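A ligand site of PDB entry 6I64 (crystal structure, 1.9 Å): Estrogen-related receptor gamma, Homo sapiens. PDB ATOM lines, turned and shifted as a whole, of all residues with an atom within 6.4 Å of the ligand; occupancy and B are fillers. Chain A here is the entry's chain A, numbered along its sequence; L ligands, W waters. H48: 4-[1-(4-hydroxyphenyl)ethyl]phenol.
Residues that only touch the ligand: Tyr 109 (2.9 Å), Ile 132 (3.4 Å), Phe 218 (3.5 Å), Leu 128 (3.5 Å), Leu 51 (3.6 Å), Ala 55 (3.6 Å), Leu 92 (3.7 Å), Met 89 (3.8 Å), Leu 54 (3.9 Å) and Ala 214 (3.98 Å).
Hydrophobic or aromatic side chains within 4 Å of the ligand: Leu 54, Ala 55, Met 89, Leu 92, Tyr 109, Leu 128, Ile 132, Ala 214 and Phe 218.
Within 4 Å of the ligand: Leu 51, Leu 54, Ala 55, Glu 58, Met 89, Leu 92, Arg 99, Tyr 109, Leu 128, Asn 129, Ile 132, Ala 214 and Phe 218.
The nearest printed residue that does not touch the ligand is Leu 125 (4.1 Å).
Water W1 lies within hydrogen-bond range of OE1 of Glu 58 (2.8 Å), O of Leu 92 (2.8 Å), OAB of the ligand (3.1 Å) and NH1 of Arg 99 (3.1 Å).
An oxygen (OAC) of the ligand lies within hydrogen-bond range of the side-chain amide nitrogen (ND2) of Asn 129 (2.9 Å).
The guanidinium group (NH2) of Arg 99 sits at hydrogen-bond distance from an oxygen (OAB) of the ligand, at 3.1 Å.
An oxygen (OAB) of the ligand sits at hydrogen-bond distance from the side-chain carboxylate (OE2) of Glu 58 (2.5 Å).
The backbone carbonyl oxygen of Tyr 109 lies within hydrogen-bond range of the guanidinium group of Arg 99, 2.9 Å away.
NE of Arg 99 lies within hydrogen-bond range of O of Val 108.
The side-chain amide nitrogen (ND2) of Asn 129 lies within hydrogen-bond range of the side-chain hydroxyl (OH) of Tyr 109, at 2.8 Å.
The guanidinium group (NH1) of Arg 99 sits close to the backbone carbonyl oxygen (O) of Gly 95 (3.4 Å).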
ATOM      1  N   LEU A  51      27.991  19.313  -6.873  1.00  0.00           N
ATOM      2  CA  LEU A  51      27.218  20.508  -7.206  1.00  0.00           C
ATOM      3  C   LEU A  51      25.902  20.156  -7.893  1.00  0.00           C
ATOM      4  O   LEU A  51      24.864  20.738  -7.563  1.00  0.00           O
ATOM      5  CB  LEU A  51      28.076  21.427  -8.079  1.00  0.00           C
ATOM      6  CG  LEU A  51      29.199  22.132  -7.304  1.00  0.00           C
ATOM      7  CD1 LEU A  51      30.262  22.613  -8.289  1.00  0.00           C
ATOM      8  CD2 LEU A  51      28.672  23.288  -6.464  1.00  0.00           C
ATOM      9  N   CYS A  52      25.918  19.234  -8.855  1.00  0.00           N
ATOM     10  CA  CYS A  52      24.656  18.856  -9.519  1.00  0.00           C
ATOM     11  C   CYS A  52      23.723  18.114  -8.563  1.00  0.00           C
ATOM     12  O   CYS A  52      22.496  18.223  -8.694  1.00  0.00           O
ATOM     13  CB  CYS A  52      24.932  17.991 -10.750  1.00  0.00           C
ATOM     14  SG  CYS A  52      25.842  18.839 -12.062  1.00  0.00           S
ATOM     15  N   LEU A  54      23.562  18.708  -5.269  1.00  0.00           N
ATOM     16  CA  LEU A  54      22.983  19.774  -4.465  1.00  0.00           C
ATOM     17  C   LEU A  54      21.884  20.493  -5.236  1.00  0.00           C
ATOM     18  O   LEU A  54      20.768  20.674  -4.738  1.00  0.00           O
ATOM     19  CB  LEU A  54      24.079  20.764  -4.045  1.00  0.00           C
ATOM     20  CG  LEU A  54      23.710  22.052  -3.305  1.00  0.00           C
ATOM     21  CD1 LEU A  54      23.128  21.721  -1.920  1.00  0.00           C
ATOM     22  CD2 LEU A  54      24.945  22.964  -3.189  1.00  0.00           C
ATOM     23  N   ALA A  55      22.180  20.873  -6.485  1.00  0.00           N
ATOM     24  CA  ALA A  55      21.205  21.609  -7.286  1.00  0.00           C
ATOM     25  C   ALA A  55      19.915  20.814  -7.446  1.00  0.00           C
ATOM     26  O   ALA A  55      18.816  21.386  -7.423  1.00  0.00           O
ATOM     27  CB  ALA A  55      21.800  21.947  -8.651  1.00  0.00           C
ATOM     28  N   GLU A  58      17.986  21.191  -4.318  1.00  0.00           N
ATOM     29  CA  GLU A  58      17.494  22.566  -4.210  1.00  0.00           C
ATOM     30  C   GLU A  58      16.324  22.813  -5.150  1.00  0.00           C
ATOM     31  O   GLU A  58      15.395  23.573  -4.800  1.00  0.00           O
ATOM     32  CB  GLU A  58      18.609  23.562  -4.491  1.00  0.00           C
ATOM     33  CG  GLU A  58      19.609  23.716  -3.361  1.00  0.00           C
ATOM     34  CD  GLU A  58      20.510  24.907  -3.584  1.00  0.00           C
ATOM     35  OE1 GLU A  58      20.023  26.047  -3.437  1.00  0.00           O
ATOM     36  OE2 GLU A  58      21.684  24.695  -3.940  1.00  0.00           O
ATOM     37  N   TRP A  88      15.025  28.365 -13.421  1.00  0.00           N
ATOM     38  CA  TRP A  88      15.606  27.561 -12.344  1.00  0.00           C
ATOM     39  C   TRP A  88      17.046  27.959 -12.037  1.00  0.00           C
ATOM     40  O   TRP A  88      17.425  28.110 -10.869  1.00  0.00           O
ATOM     41  CB  TRP A  88      15.505  26.061 -12.677  1.00  0.00           C
ATOM     42  CG  TRP A  88      16.278  25.619 -13.888  1.00  0.00           C
ATOM     43  CD1 TRP A  88      15.881  25.711 -15.184  1.00  0.00           C
ATOM     44  CD2 TRP A  88      17.565  24.984 -13.899  1.00  0.00           C
ATOM     45  NE1 TRP A  88      16.847  25.188 -16.016  1.00  0.00           N
ATOM     46  CE2 TRP A  88      17.892  24.742 -15.249  1.00  0.00           C
ATOM     47  CE3 TRP A  88      18.474  24.607 -12.898  1.00  0.00           C
ATOM     48  CZ2 TRP A  88      19.087  24.115 -15.629  1.00  0.00           C
ATOM     49  CZ3 TRP A  88      19.664  24.000 -13.286  1.00  0.00           C
ATOM     50  CH2 TRP A  88      19.962  23.763 -14.628  1.00  0.00           C
ATOM     51  N   MET A  89      17.864  28.164 -13.078  1.00  0.00           N
ATOM     52  CA  MET A  89      19.284  28.431 -12.875  1.00  0.00           C
ATOM     53  C   MET A  89      19.510  29.828 -12.308  1.00  0.00           C
ATOM     54  O   MET A  89      20.391  30.018 -11.453  1.00  0.00           O
ATOM     55  CB  MET A  89      20.043  28.235 -14.183  1.00  0.00           C
ATOM     56  CG  MET A  89      21.554  28.437 -14.101  1.00  0.00           C
ATOM     57  SD  MET A  89      22.403  27.288 -12.984  1.00  0.00           S
ATOM     58  CE  MET A  89      22.736  25.884 -14.067  1.00  0.00           C
ATOM     59  N   LEU A  92      18.809  29.447  -8.623  1.00  0.00           N
ATOM     60  CA  LEU A  92      19.920  28.798  -7.950  1.00  0.00           C
ATOM     61  C   LEU A  92      21.084  29.760  -7.792  1.00  0.00           C
ATOM     62  O   LEU A  92      21.645  29.896  -6.693  1.00  0.00           O
ATOM     63  CB  LEU A  92      20.352  27.550  -8.732  1.00  0.00           C
ATOM     64  CG  LEU A  92      19.484  26.285  -8.630  1.00  0.00           C
ATOM     65  CD1 LEU A  92      19.942  25.218  -9.621  1.00  0.00           C
ATOM     66  CD2 LEU A  92      19.505  25.729  -7.205  1.00  0.00           C
ATOM     67  N   ILE A  93      21.456  30.465  -8.863  1.00  0.00           N
ATOM     68  CA  ILE A  93      22.631  31.337  -8.811  1.00  0.00           C
ATOM     69  C   ILE A  93      22.400  32.486  -7.856  1.00  0.00           C
ATOM     70  O   ILE A  93      23.290  32.853  -7.072  1.00  0.00           O
ATOM     71  CB  ILE A  93      23.004  31.835 -10.223  1.00  0.00           C
ATOM     72  CG1 ILE A  93      23.661  30.678 -11.013  1.00  0.00           C
ATOM     73  CG2 ILE A  93      23.932  33.064 -10.129  1.00  0.00           C
ATOM     74  CD1 ILE A  93      24.030  31.039 -12.473  1.00  0.00           C
ATOM     75  N   GLY A  95      20.748  32.402  -5.241  1.00  0.00           N
ATOM     76  CA  GLY A  95      20.953  31.820  -3.914  1.00  0.00           C
ATOM     77  C   GLY A  95      22.410  31.818  -3.477  1.00  0.00           C
ATOM     78  O   GLY A  95      22.729  32.304  -2.398  1.00  0.00           O
ATOM     79  N   VAL A  96      23.295  31.253  -4.300  1.00  0.00           N
ATOM     80  CA  VAL A  96      24.694  31.191  -3.878  1.00  0.00           C
ATOM     81  C   VAL A  96      25.279  32.607  -3.805  1.00  0.00           C
ATOM     82  O   VAL A  96      26.086  32.894  -2.925  1.00  0.00           O
ATOM     83  CB  VAL A  96      25.516  30.263  -4.790  1.00  0.00           C
ATOM     84  CG1 VAL A  96      25.465  30.715  -6.265  1.00  0.00           C
ATOM     85  CG2 VAL A  96      26.979  30.171  -4.311  1.00  0.00           C
ATOM     86  N   ARG A  99      24.239  33.940  -0.364  1.00  0.00           N
ATOM     87  CA  ARG A  99      24.985  33.287   0.712  1.00  0.00           C
ATOM     88  C   ARG A  99      26.439  33.710   0.768  1.00  0.00           C
ATOM     89  O   ARG A  99      27.101  33.510   1.788  1.00  0.00           O
ATOM     90  CB  ARG A  99      24.903  31.770   0.577  1.00  0.00           C
ATOM     91  CG  ARG A  99      23.497  31.234   0.553  1.00  0.00           C
ATOM     92  CD  ARG A  99      23.485  29.731   0.714  1.00  0.00           C
ATOM     93  NE  ARG A  99      23.859  29.004  -0.506  1.00  0.00           N
ATOM     94  CZ  ARG A  99      23.030  28.753  -1.528  1.00  0.00           C
ATOM     95  NH1 ARG A  99      21.791  29.199  -1.533  1.00  0.00           N
ATOM     96  NH2 ARG A  99      23.455  28.049  -2.562  1.00  0.00           N
ATOM     97  N   LEU A 107      32.637  31.303  -2.898  1.00  0.00           N
ATOM     98  CA  LEU A 107      31.233  31.050  -3.211  1.00  0.00           C
ATOM     99  C   LEU A 107      30.689  30.009  -2.266  1.00  0.00           C
ATOM    100  O   LEU A 107      31.189  28.876  -2.214  1.00  0.00           O
ATOM    101  CB  LEU A 107      31.067  30.609  -4.668  1.00  0.00           C
ATOM    102  CG  LEU A 107      31.358  31.715  -5.682  1.00  0.00           C
ATOM    103  CD1 LEU A 107      31.072  31.204  -7.112  1.00  0.00           C
ATOM    104  CD2 LEU A 107      30.542  32.952  -5.354  1.00  0.00           C
ATOM    105  N   VAL A 108      29.656  30.386  -1.504  1.00  0.00           N
ATOM    106  CA  VAL A 108      29.085  29.513  -0.471  1.00  0.00           C
ATOM    107  C   VAL A 108      27.928  28.762  -1.105  1.00  0.00           C
ATOM    108  O   VAL A 108      26.752  29.136  -0.975  1.00  0.00           O
ATOM    109  CB  VAL A 108      28.657  30.325   0.770  1.00  0.00           C
ATOM    110  CG1 VAL A 108      28.072  29.425   1.875  1.00  0.00           C
ATOM    111  CG2 VAL A 108      29.840  31.146   1.307  1.00  0.00           C
ATOM    112  N   TYR A 109      28.248  27.669  -1.809  1.00  0.00           N
ATOM    113  CA  TYR A 109      27.178  26.819  -2.361  1.00  0.00           C
ATOM    114  C   TYR A 109      26.366  26.202  -1.230  1.00  0.00           C
ATOM    115  O   TYR A 109      25.138  26.064  -1.339  1.00  0.00           O
ATOM    116  CB  TYR A 109      27.771  25.740  -3.266  1.00  0.00           C
ATOM    117  CG  TYR A 109      28.254  26.307  -4.580  1.00  0.00           C
ATOM    118  CD1 TYR A 109      27.381  26.479  -5.645  1.00  0.00           C
ATOM    119  CD2 TYR A 109      29.568  26.750  -4.720  1.00  0.00           C
ATOM    120  CE1 TYR A 109      27.812  27.045  -6.845  1.00  0.00           C
ATOM    121  CE2 TYR A 109      30.012  27.304  -5.904  1.00  0.00           C
ATOM    122  CZ  TYR A 109      29.137  27.450  -6.961  1.00  0.00           C
ATOM    123  OH  TYR A 109      29.579  28.011  -8.126  1.00  0.00           O
ATOM    124  N   MET A 115      33.611  27.322  -2.136  1.00  0.00           N
ATOM    125  CA  MET A 115      34.603  27.181  -3.206  1.00  0.00           C
ATOM    126  C   MET A 115      35.476  28.422  -3.310  1.00  0.00           C
ATOM    127  O   MET A 115      34.955  29.531  -3.482  1.00  0.00           O
ATOM    128  CB  MET A 115      33.934  26.917  -4.553  1.00  0.00           C
ATOM    129  CG  MET A 115      33.300  25.538  -4.705  1.00  0.00           C
ATOM    130  SD  MET A 115      32.697  25.227  -6.392  1.00  0.00           S
ATOM    131  CE  MET A 115      34.230  25.235  -7.270  1.00  0.00           C
ATOM    132  N   LEU A 125      35.457  25.434 -13.459  1.00  0.00           N
ATOM    133  CA  LEU A 125      34.403  26.432 -13.253  1.00  0.00           C
ATOM    134  C   LEU A 125      34.961  27.831 -13.017  1.00  0.00           C
ATOM    135  O   LEU A 125      34.222  28.722 -12.564  1.00  0.00           O
ATOM    136  CB  LEU A 125      33.513  26.019 -12.069  1.00  0.00           C
ATOM    137  CG  LEU A 125      32.623  24.785 -12.297  1.00  0.00           C
ATOM    138  CD1 LEU A 125      32.022  24.268 -10.976  1.00  0.00           C
ATOM    139  CD2 LEU A 125      31.519  25.097 -13.298  1.00  0.00           C
ATOM    140  N   LEU A 128      32.999  30.637 -14.976  1.00  0.00           N
ATOM    141  CA  LEU A 128      31.621  30.772 -14.521  1.00  0.00           C
ATOM    142  C   LEU A 128      31.562  31.332 -13.097  1.00  0.00           C
ATOM    143  O   LEU A 128      30.758  32.225 -12.808  1.00  0.00           O
ATOM    144  CB  LEU A 128      30.903  29.423 -14.583  1.00  0.00           C
ATOM    145  CG  LEU A 128      30.066  29.105 -15.825  1.00  0.00           C
ATOM    146  CD1 LEU A 128      29.374  27.759 -15.653  1.00  0.00           C
ATOM    147  CD2 LEU A 128      29.039  30.210 -16.153  1.00  0.00           C
ATOM    148  N   ASN A 129      32.416  30.829 -12.215  1.00  0.00           N
ATOM    149  CA  ASN A 129      32.400  31.324 -10.839  1.00  0.00           C
ATOM    150  C   ASN A 129      32.881  32.769 -10.772  1.00  0.00           C
ATOM    151  O   ASN A 129      32.417  33.534  -9.920  1.00  0.00           O
ATOM    152  CB  ASN A 129      33.276  30.445  -9.953  1.00  0.00           C
ATOM    153  CG  ASN A 129      32.574  29.168  -9.518  1.00  0.00           C
ATOM    154  OD1 ASN A 129      33.085  28.430  -8.681  1.00  0.00           O
ATOM    155  ND2 ASN A 129      31.410  28.904 -10.089  1.00  0.00           N
ATOM    156  N   ILE A 132      29.878  34.777 -11.350  1.00  0.00           N
ATOM    157  CA  ILE A 132      29.053  34.781 -10.159  1.00  0.00           C
ATOM    158  C   ILE A 132      29.643  35.723  -9.127  1.00  0.00           C
ATOM    159  O   ILE A 132      28.918  36.444  -8.423  1.00  0.00           O
ATOM    160  CB  ILE A 132      28.908  33.338  -9.614  1.00  0.00           C
ATOM    161  CG1 ILE A 132      28.104  32.531 -10.632  1.00  0.00           C
ATOM    162  CG2 ILE A 132      28.260  33.320  -8.246  1.00  0.00           C
ATOM    163  CD1 ILE A 132      28.085  31.031 -10.377  1.00  0.00           C
ATOM    164  N   ALA A 214      25.810  29.358 -17.627  1.00  0.00           N
ATOM    165  CA  ALA A 214      25.887  28.210 -16.714  1.00  0.00           C
ATOM    166  C   ALA A 214      25.073  27.028 -17.232  1.00  0.00           C
ATOM    167  O   ALA A 214      25.544  25.883 -17.177  1.00  0.00           O
ATOM    168  CB  ALA A 214      25.416  28.609 -15.312  1.00  0.00           C
ATOM    169  N   PHE A 218      26.623  23.302 -18.104  1.00  0.00           N
ATOM    170  CA  PHE A 218      26.242  22.031 -17.505  1.00  0.00           C
ATOM    171  C   PHE A 218      25.518  21.150 -18.503  1.00  0.00           C
ATOM    172  O   PHE A 218      25.550  19.925 -18.351  1.00  0.00           O
ATOM    173  CB  PHE A 218      25.409  22.259 -16.234  1.00  0.00           C
ATOM    174  CG  PHE A 218      26.261  22.637 -15.053  1.00  0.00           C
ATOM    175  CD1 PHE A 218      26.848  21.666 -14.268  1.00  0.00           C
ATOM    176  CD2 PHE A 218      26.534  23.965 -14.767  1.00  0.00           C
ATOM    177  CE1 PHE A 218      27.666  22.004 -13.213  1.00  0.00           C
ATOM    178  CE2 PHE A 218      27.357  24.316 -13.695  1.00  0.00           C
ATOM    179  CZ  PHE A 218      27.923  23.336 -12.919  1.00  0.00           C
ATOM    180  N   PHE A 233      17.217  17.504 -12.095  1.00  0.00           N
ATOM    181  CA  PHE A 233      18.242  18.344 -12.698  1.00  0.00           C
ATOM    182  C   PHE A 233      18.331  18.094 -14.196  1.00  0.00           C
ATOM    183  O   PHE A 233      18.410  19.042 -14.976  1.00  0.00           O
ATOM    184  CB  PHE A 233      19.587  18.083 -12.019  1.00  0.00           C
ATOM    185  CG  PHE A 233      20.680  19.028 -12.410  1.00  0.00           C
ATOM    186  CD1 PHE A 233      20.775  20.289 -11.814  1.00  0.00           C
ATOM    187  CD2 PHE A 233      21.646  18.643 -13.322  1.00  0.00           C
ATOM    188  CE1 PHE A 233      21.803  21.163 -12.163  1.00  0.00           C
ATOM    189  CE2 PHE A 233      22.674  19.501 -13.676  1.00  0.00           C
ATOM    190  CZ  PHE A 233      22.763  20.749 -13.097  1.00  0.00           C
HETATM  191  CAA H48 L   1      24.279  24.433 -10.948  1.00  0.00           C
HETATM  192  CAD H48 L   1      23.817  26.987  -7.304  1.00  0.00           C
HETATM  193  CAE H48 L   1      23.782  24.697  -6.510  1.00  0.00           C
HETATM  194  CAF H48 L   1      28.547  26.381 -10.356  1.00  0.00           C
HETATM  195  CAG H48 L   1      26.946  27.432 -11.833  1.00  0.00           C
HETATM  196  CAH H48 L   1      24.413  26.555  -8.508  1.00  0.00           C
HETATM  197  CAI H48 L   1      24.379  24.282  -7.709  1.00  0.00           C
HETATM  198  CAJ H48 L   1      27.567  25.529  -9.885  1.00  0.00           C
HETATM  199  CAK H48 L   1      25.965  26.567 -11.357  1.00  0.00           C
HETATM  200  CAL H48 L   1      23.501  26.053  -6.298  1.00  0.00           C
HETATM  201  CAM H48 L   1      28.242  27.329 -11.318  1.00  0.00           C
HETATM  202  CAN H48 L   1      24.700  25.199  -8.698  1.00  0.00           C
HETATM  203  CAO H48 L   1      26.275  25.619 -10.373  1.00  0.00           C
HETATM  204  CAP H48 L   1      25.313  24.719  -9.884  1.00  0.00           C
HETATM  205  OAB H48 L   1      22.906  26.458  -5.127  1.00  0.00           O
HETATM  206  OAC H48 L   1      29.217  28.150 -11.748  1.00  0.00           O
HETATM  207  O   HOH W   1      20.775  28.532  -4.362  1.00  0.00           O
